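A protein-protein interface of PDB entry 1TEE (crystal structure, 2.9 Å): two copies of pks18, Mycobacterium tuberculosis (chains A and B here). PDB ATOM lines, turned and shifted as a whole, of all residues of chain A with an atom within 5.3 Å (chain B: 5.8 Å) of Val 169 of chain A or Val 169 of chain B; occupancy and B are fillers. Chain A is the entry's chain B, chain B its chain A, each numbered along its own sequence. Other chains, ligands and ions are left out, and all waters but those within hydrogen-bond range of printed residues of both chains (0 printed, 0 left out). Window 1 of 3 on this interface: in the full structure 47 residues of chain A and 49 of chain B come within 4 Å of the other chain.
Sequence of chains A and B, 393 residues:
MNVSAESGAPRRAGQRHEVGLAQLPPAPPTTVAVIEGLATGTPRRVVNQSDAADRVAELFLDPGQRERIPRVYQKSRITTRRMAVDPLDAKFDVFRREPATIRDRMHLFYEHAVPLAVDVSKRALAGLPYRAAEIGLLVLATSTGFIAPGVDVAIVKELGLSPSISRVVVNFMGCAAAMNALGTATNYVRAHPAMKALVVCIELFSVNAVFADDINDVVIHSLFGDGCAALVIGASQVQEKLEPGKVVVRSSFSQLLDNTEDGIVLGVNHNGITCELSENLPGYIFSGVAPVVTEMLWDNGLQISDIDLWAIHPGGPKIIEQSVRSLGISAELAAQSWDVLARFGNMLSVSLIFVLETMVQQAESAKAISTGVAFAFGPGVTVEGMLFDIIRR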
ATOM      1  N   LEU A 140      33.283  27.437 -27.325  1.00  0.00           N
ATOM      2  CA  LEU A 140      32.488  28.629 -27.591  1.00  0.00           C
ATOM      3  C   LEU A 140      31.601  28.914 -26.392  1.00  0.00           C
ATOM      4  O   LEU A 140      30.801  28.065 -25.986  1.00  0.00           O
ATOM      5  CB  LEU A 140      31.629  28.407 -28.841  1.00  0.00           C
ATOM      6  CG  LEU A 140      30.788  29.527 -29.481  1.00  0.00           C
ATOM      7  CD1 LEU A 140      29.669  29.945 -28.550  1.00  0.00           C
ATOM      8  CD2 LEU A 140      31.677  30.707 -29.828  1.00  0.00           C
ATOM      9  N   ASP A 152      29.841  28.188 -33.375  1.00  0.00           N
ATOM     10  CA  ASP A 152      30.979  27.284 -33.367  1.00  0.00           C
ATOM     11  C   ASP A 152      31.134  26.651 -34.751  1.00  0.00           C
ATOM     12  O   ASP A 152      32.222  26.670 -35.324  1.00  0.00           O
ATOM     13  CB  ASP A 152      30.826  26.215 -32.268  1.00  0.00           C
ATOM     14  CG  ASP A 152      29.681  25.243 -32.533  1.00  0.00           C
ATOM     15  OD1 ASP A 152      28.563  25.694 -32.875  1.00  0.00           O
ATOM     16  OD2 ASP A 152      29.895  24.021 -32.388  1.00  0.00           O
ATOM     17  N   ARG A 167      34.748  20.073 -30.297  1.00  0.00           N
ATOM     18  CA  ARG A 167      33.980  21.267 -29.979  1.00  0.00           C
ATOM     19  C   ARG A 167      33.186  21.171 -28.684  1.00  0.00           C
ATOM     20  O   ARG A 167      32.571  20.156 -28.389  1.00  0.00           O
ATOM     21  CB  ARG A 167      33.054  21.603 -31.148  1.00  0.00           C
ATOM     22  CG  ARG A 167      33.801  22.189 -32.314  1.00  0.00           C
ATOM     23  CD  ARG A 167      32.881  22.686 -33.407  1.00  0.00           C
ATOM     24  NE  ARG A 167      32.266  21.589 -34.145  1.00  0.00           N
ATOM     25  CZ  ARG A 167      31.137  20.983 -33.801  1.00  0.00           C
ATOM     26  NH1 ARG A 167      30.473  21.364 -32.718  1.00  0.00           N
ATOM     27  NH2 ARG A 167      30.674  19.991 -34.543  1.00  0.00           N
ATOM     28  N   VAL A 168      33.220  22.241 -27.905  1.00  0.00           N
ATOM     29  CA  VAL A 168      32.476  22.298 -26.655  1.00  0.00           C
ATOM     30  C   VAL A 168      31.798  23.659 -26.581  1.00  0.00           C
ATOM     31  O   VAL A 168      32.477  24.692 -26.610  1.00  0.00           O
ATOM     32  CB  VAL A 168      33.398  22.160 -25.432  1.00  0.00           C
ATOM     33  CG1 VAL A 168      32.576  22.149 -24.169  1.00  0.00           C
ATOM     34  CG2 VAL A 168      34.218  20.903 -25.540  1.00  0.00           C
ATOM     35  N   VAL A 169      30.468  23.660 -26.504  1.00  0.00           N
ATOM     36  CA  VAL A 169      29.721  24.906 -26.398  1.00  0.00           C
ATOM     37  C   VAL A 169      29.325  25.156 -24.946  1.00  0.00           C
ATOM     38  O   VAL A 169      28.485  24.448 -24.394  1.00  0.00           O
ATOM     39  CB  VAL A 169      28.460  24.878 -27.243  1.00  0.00           C
ATOM     40  CG1 VAL A 169      27.721  26.190 -27.080  1.00  0.00           C
ATOM     41  CG2 VAL A 169      28.816  24.657 -28.691  1.00  0.00           C
ATOM     42  N   VAL A 170      29.929  26.174 -24.341  1.00  0.00           N
ATOM     43  CA  VAL A 170      29.676  26.527 -22.947  1.00  0.00           C
ATOM     44  C   VAL A 170      28.610  27.609 -22.759  1.00  0.00           C
ATOM     45  O   VAL A 170      28.895  28.798 -22.907  1.00  0.00           O
ATOM     46  CB  VAL A 170      30.969  27.010 -22.282  1.00  0.00           C
ATOM     47  CG1 VAL A 170      30.742  27.255 -20.816  1.00  0.00           C
ATOM     48  CG2 VAL A 170      32.051  25.981 -22.486  1.00  0.00           C
ATOM     49  N   ASN A 171      27.396  27.188 -22.400  1.00  0.00           N
ATOM     50  CA  ASN A 171      26.273  28.104 -22.191  1.00  0.00           C
ATOM     51  C   ASN A 171      25.891  28.424 -20.737  1.00  0.00           C
ATOM     52  O   ASN A 171      26.100  27.637 -19.813  1.00  0.00           O
ATOM     53  CB  ASN A 171      25.019  27.571 -22.894  1.00  0.00           C
ATOM     54  CG  ASN A 171      24.987  27.897 -24.363  1.00  0.00           C
ATOM     55  OD1 ASN A 171      24.912  29.066 -24.742  1.00  0.00           O
ATOM     56  ND2 ASN A 171      25.035  26.866 -25.207  1.00  0.00           N
ATOM     57  N   MET A 173      26.997  30.341 -18.302  1.00  0.00           N
ATOM     58  CA  MET A 173      27.886  30.419 -17.153  1.00  0.00           C
ATOM     59  C   MET A 173      28.177  31.893 -16.886  1.00  0.00           C
ATOM     60  O   MET A 173      29.054  32.243 -16.098  1.00  0.00           O
ATOM     61  CB  MET A 173      29.159  29.606 -17.394  1.00  0.00           C
ATOM     62  CG  MET A 173      28.837  28.141 -17.614  1.00  0.00           C
ATOM     63  SD  MET A 173      30.128  26.992 -17.191  1.00  0.00           S
ATOM     64  CE  MET A 173      29.871  26.791 -15.423  1.00  0.00           C
ATOM     65  N   LEU B 138      33.059  18.648 -12.850  1.00  0.00           N
ATOM     66  CA  LEU B 138      31.681  18.216 -13.009  1.00  0.00           C
ATOM     67  C   LEU B 138      31.243  18.764 -14.358  1.00  0.00           C
ATOM     68  O   LEU B 138      31.388  19.948 -14.631  1.00  0.00           O
ATOM     69  CB  LEU B 138      30.804  18.766 -11.875  1.00  0.00           C
ATOM     70  CG  LEU B 138      29.279  18.735 -12.055  1.00  0.00           C
ATOM     71  CD1 LEU B 138      28.830  17.460 -12.720  1.00  0.00           C
ATOM     72  CD2 LEU B 138      28.617  18.865 -10.721  1.00  0.00           C
ATOM     73  N   VAL B 139      30.742  17.892 -15.215  1.00  0.00           N
ATOM     74  CA  VAL B 139      30.308  18.307 -16.530  1.00  0.00           C
ATOM     75  C   VAL B 139      28.829  18.001 -16.630  1.00  0.00           C
ATOM     76  O   VAL B 139      28.405  16.887 -16.342  1.00  0.00           O
ATOM     77  CB  VAL B 139      31.069  17.538 -17.634  1.00  0.00           C
ATOM     78  CG1 VAL B 139      30.709  18.095 -19.011  1.00  0.00           C
ATOM     79  CG2 VAL B 139      32.570  17.631 -17.389  1.00  0.00           C
ATOM     80  N   LEU B 140      28.042  18.995 -17.034  1.00  0.00           N
ATOM     81  CA  LEU B 140      26.606  18.819 -17.155  1.00  0.00           C
ATOM     82  C   LEU B 140      26.169  19.171 -18.566  1.00  0.00           C
ATOM     83  O   LEU B 140      26.423  20.275 -19.043  1.00  0.00           O
ATOM     84  CB  LEU B 140      25.891  19.711 -16.139  1.00  0.00           C
ATOM     85  CG  LEU B 140      24.415  19.474 -15.789  1.00  0.00           C
ATOM     86  CD1 LEU B 140      23.531  19.683 -17.021  1.00  0.00           C
ATOM     87  CD2 LEU B 140      24.247  18.068 -15.214  1.00  0.00           C
ATOM     88  N   ALA B 141      25.511  18.227 -19.230  1.00  0.00           N
ATOM     89  CA  ALA B 141      25.040  18.442 -20.591  1.00  0.00           C
ATOM     90  C   ALA B 141      23.513  18.353 -20.685  1.00  0.00           C
ATOM     91  O   ALA B 141      22.889  17.493 -20.052  1.00  0.00           O
ATOM     92  CB  ALA B 141      25.692  17.421 -21.526  1.00  0.00           C
ATOM     93  N   ASP B 152      23.717  21.820 -12.145  1.00  0.00           N
ATOM     94  CA  ASP B 152      25.125  21.655 -11.796  1.00  0.00           C
ATOM     95  C   ASP B 152      25.412  22.083 -10.359  1.00  0.00           C
ATOM     96  O   ASP B 152      26.071  21.355  -9.619  1.00  0.00           O
ATOM     97  CB  ASP B 152      26.024  22.427 -12.776  1.00  0.00           C
ATOM     98  CG  ASP B 152      25.837  23.945 -12.711  1.00  0.00           C
ATOM     99  OD1 ASP B 152      24.683  24.427 -12.711  1.00  0.00           O
ATOM    100  OD2 ASP B 152      26.858  24.664 -12.686  1.00  0.00           O
ATOM    101  N   ARG B 167      33.393  23.354 -12.920  1.00  0.00           N
ATOM    102  CA  ARG B 167      32.159  23.026 -13.600  1.00  0.00           C
ATOM    103  C   ARG B 167      32.092  23.565 -15.011  1.00  0.00           C
ATOM    104  O   ARG B 167      32.539  24.672 -15.304  1.00  0.00           O
ATOM    105  CB  ARG B 167      30.983  23.521 -12.766  1.00  0.00           C
ATOM    106  CG  ARG B 167      31.012  22.906 -11.378  1.00  0.00           C
ATOM    107  CD  ARG B 167      29.943  23.420 -10.452  1.00  0.00           C
ATOM    108  NE  ARG B 167      30.183  24.799 -10.046  1.00  0.00           N
ATOM    109  CZ  ARG B 167      29.683  25.855 -10.672  1.00  0.00           C
ATOM    110  NH1 ARG B 167      28.908  25.696 -11.733  1.00  0.00           N
ATOM    111  NH2 ARG B 167      29.968  27.067 -10.234  1.00  0.00           N
ATOM    112  N   VAL B 168      31.549  22.737 -15.889  1.00  0.00           N
ATOM    113  CA  VAL B 168      31.379  23.075 -17.285  1.00  0.00           C
ATOM    114  C   VAL B 168      29.970  22.662 -17.645  1.00  0.00           C
ATOM    115  O   VAL B 168      29.555  21.538 -17.363  1.00  0.00           O
ATOM    116  CB  VAL B 168      32.332  22.281 -18.192  1.00  0.00           C
ATOM    117  CG1 VAL B 168      32.191  22.765 -19.626  1.00  0.00           C
ATOM    118  CG2 VAL B 168      33.758  22.420 -17.699  1.00  0.00           C
ATOM    119  N   VAL B 169      29.223  23.572 -18.252  1.00  0.00           N
ATOM    120  CA  VAL B 169      27.870  23.246 -18.663  1.00  0.00           C
ATOM    121  C   VAL B 169      27.860  23.217 -20.178  1.00  0.00           C
ATOM    122  O   VAL B 169      28.255  24.178 -20.840  1.00  0.00           O
ATOM    123  CB  VAL B 169      26.837  24.280 -18.136  1.00  0.00           C
ATOM    124  CG1 VAL B 169      25.511  24.108 -18.862  1.00  0.00           C
ATOM    125  CG2 VAL B 169      26.630  24.084 -16.643  1.00  0.00           C
ATOM    126  N   VAL B 170      27.424  22.096 -20.726  1.00  0.00           N
ATOM    127  CA  VAL B 170      27.382  21.951 -22.160  1.00  0.00           C
ATOM    128  C   VAL B 170      25.942  21.958 -22.608  1.00  0.00           C
ATOM    129  O   VAL B 170      25.168  21.086 -22.234  1.00  0.00           O
ATOM    130  CB  VAL B 170      28.047  20.648 -22.588  1.00  0.00           C
ATOM    131  CG1 VAL B 170      28.174  20.610 -24.099  1.00  0.00           C
ATOM    132  CG2 VAL B 170      29.410  20.526 -21.913  1.00  0.00           C
ATOM    133  N   ASN B 171      25.582  22.946 -23.412  1.00  0.00           N
ATOM    134  CA  ASN B 171      24.219  23.045 -23.881  1.00  0.00           C
ATOM    135  C   ASN B 171      24.069  22.932 -25.382  1.00  0.00           C
ATOM    136  O   ASN B 171      25.023  23.118 -26.126  1.00  0.00           O
ATOM    137  CB  ASN B 171      23.600  24.359 -23.402  1.00  0.00           C
ATOM    138  CG  ASN B 171      23.299  24.342 -21.928  1.00  0.00           C
ATOM    139  OD1 ASN B 171      22.609  23.453 -21.451  1.00  0.00           O
ATOM    140  ND2 ASN B 171      23.811  25.318 -21.196  1.00  0.00           N
ATOM    141  N   MET B 173      24.094  20.685 -27.585  1.00  0.00           N
ATOM    142  CA  MET B 173      24.984  19.897 -28.424  1.00  0.00           C
ATOM    143  C   MET B 173      24.268  18.647 -28.918  1.00  0.00           C
ATOM    144  O   MET B 173      24.857  17.777 -29.547  1.00  0.00           O
ATOM    145  CB  MET B 173      26.278  19.560 -27.681  1.00  0.00           C
ATOM    146  CG  MET B 173      27.143  20.788 -27.460  1.00  0.00           C
ATOM    147  SD  MET B 173      28.909  20.476 -27.357  1.00  0.00           S
ATOM    148  CE  MET B 173      29.352  20.403 -29.107  1.00  0.00           C
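Hydrophobic or aromatic side chains of chain A that line the printed part of chain B: Val 170 and Met 173.
Hydrophobic or aromatic side chains of chain B within 4 Å of the printed part of chain A: Val 169, Val 170 and Met 173.
Among the printed residues, 10 pairs touch across the chains.
Among the printed residues, no Asp or Glu carboxylate lies within 4 Å of a Lys or Arg side-chain nitrogen of the other chain.
The backbone carbonyl oxygen (O) of Val 169 of chain B lies within hydrogen-bond range of the backbone NH (N) of Asn 171 of chain A, at 3.5 Å.
SD of Met 173 of chain A is in hydrogen-bond range of N of Val 169 of chain B.
N of Asn 171 of chain B sits at hydrogen-bond distance from O of Val 169 of chain A (3.4 Å).
SD of Met 173 of chain B is in hydrogen-bond range of N of Val 169 of chain A (3.6 Å).
The backbone NH of Val 170 of chain B is in hydrogen-bond range of the backbone carbonyl oxygen of Leu 140 of chain B, at 2.7 Å.
NH1 of Arg 167 of chain B lies within salt-bridge range of OD2 of Asp 152 of chain B, at 2.5 Å.
The backbone NH of Val 170 of chain A lies within hydrogen-bond range of the backbone carbonyl oxygen of Leu 140 of chain A, 2.7 Å away.
The side-chain carboxylate of Asp 152 of chain A lies within salt-bridge range of the guanidinium group of Arg 167 of chain A, at 2.7 Å.
Val 169 of chain B touches its own counterpart, Val 169 of chain A.
Val 169 of chain A touches Val 170 of chain B, and with the chains exchanged Val 170 of chain A touches Val 169 of chain B.
Val 169 of chain A touches Asn 171 of chain B, and with the chains exchanged Asn 171 of chain A touches Val 169 of chain B.
Asn 171 of chain A touches its own counterpart, Asn 171 of chain B.
Among the printed residues, pairs that only touch across the chains: Arg 167 of chain A with Met 173 of chain B, Val 169 of chain A with Val 169 of chain B, Val 169 of chain A with Val 170 of chain B, Val 170 of chain A with Val 169 of chain B, Asn 171 of chain A with Asn 171 of chain B and Met 173 of chain A with Arg 167 of chain B.
Val 168 of chain A touches none of the printed residues of chain B.
Of the printed residues of chain B, Val 169 of chain A touches Val 169, Val 170, Asn 171 and Met 173.
Printed residues of chain B within 4 Å of Asn 171 of chain A: Val 169 (3.5 Å) and Asn 171 (3.1 Å).
Of the printed residues of chain A, Val 170 of chain B touches Val 169.
The nearest printed residue of chain A that does not touch Met 173 of chain B is Val 168 of chain A (4.1 Å).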
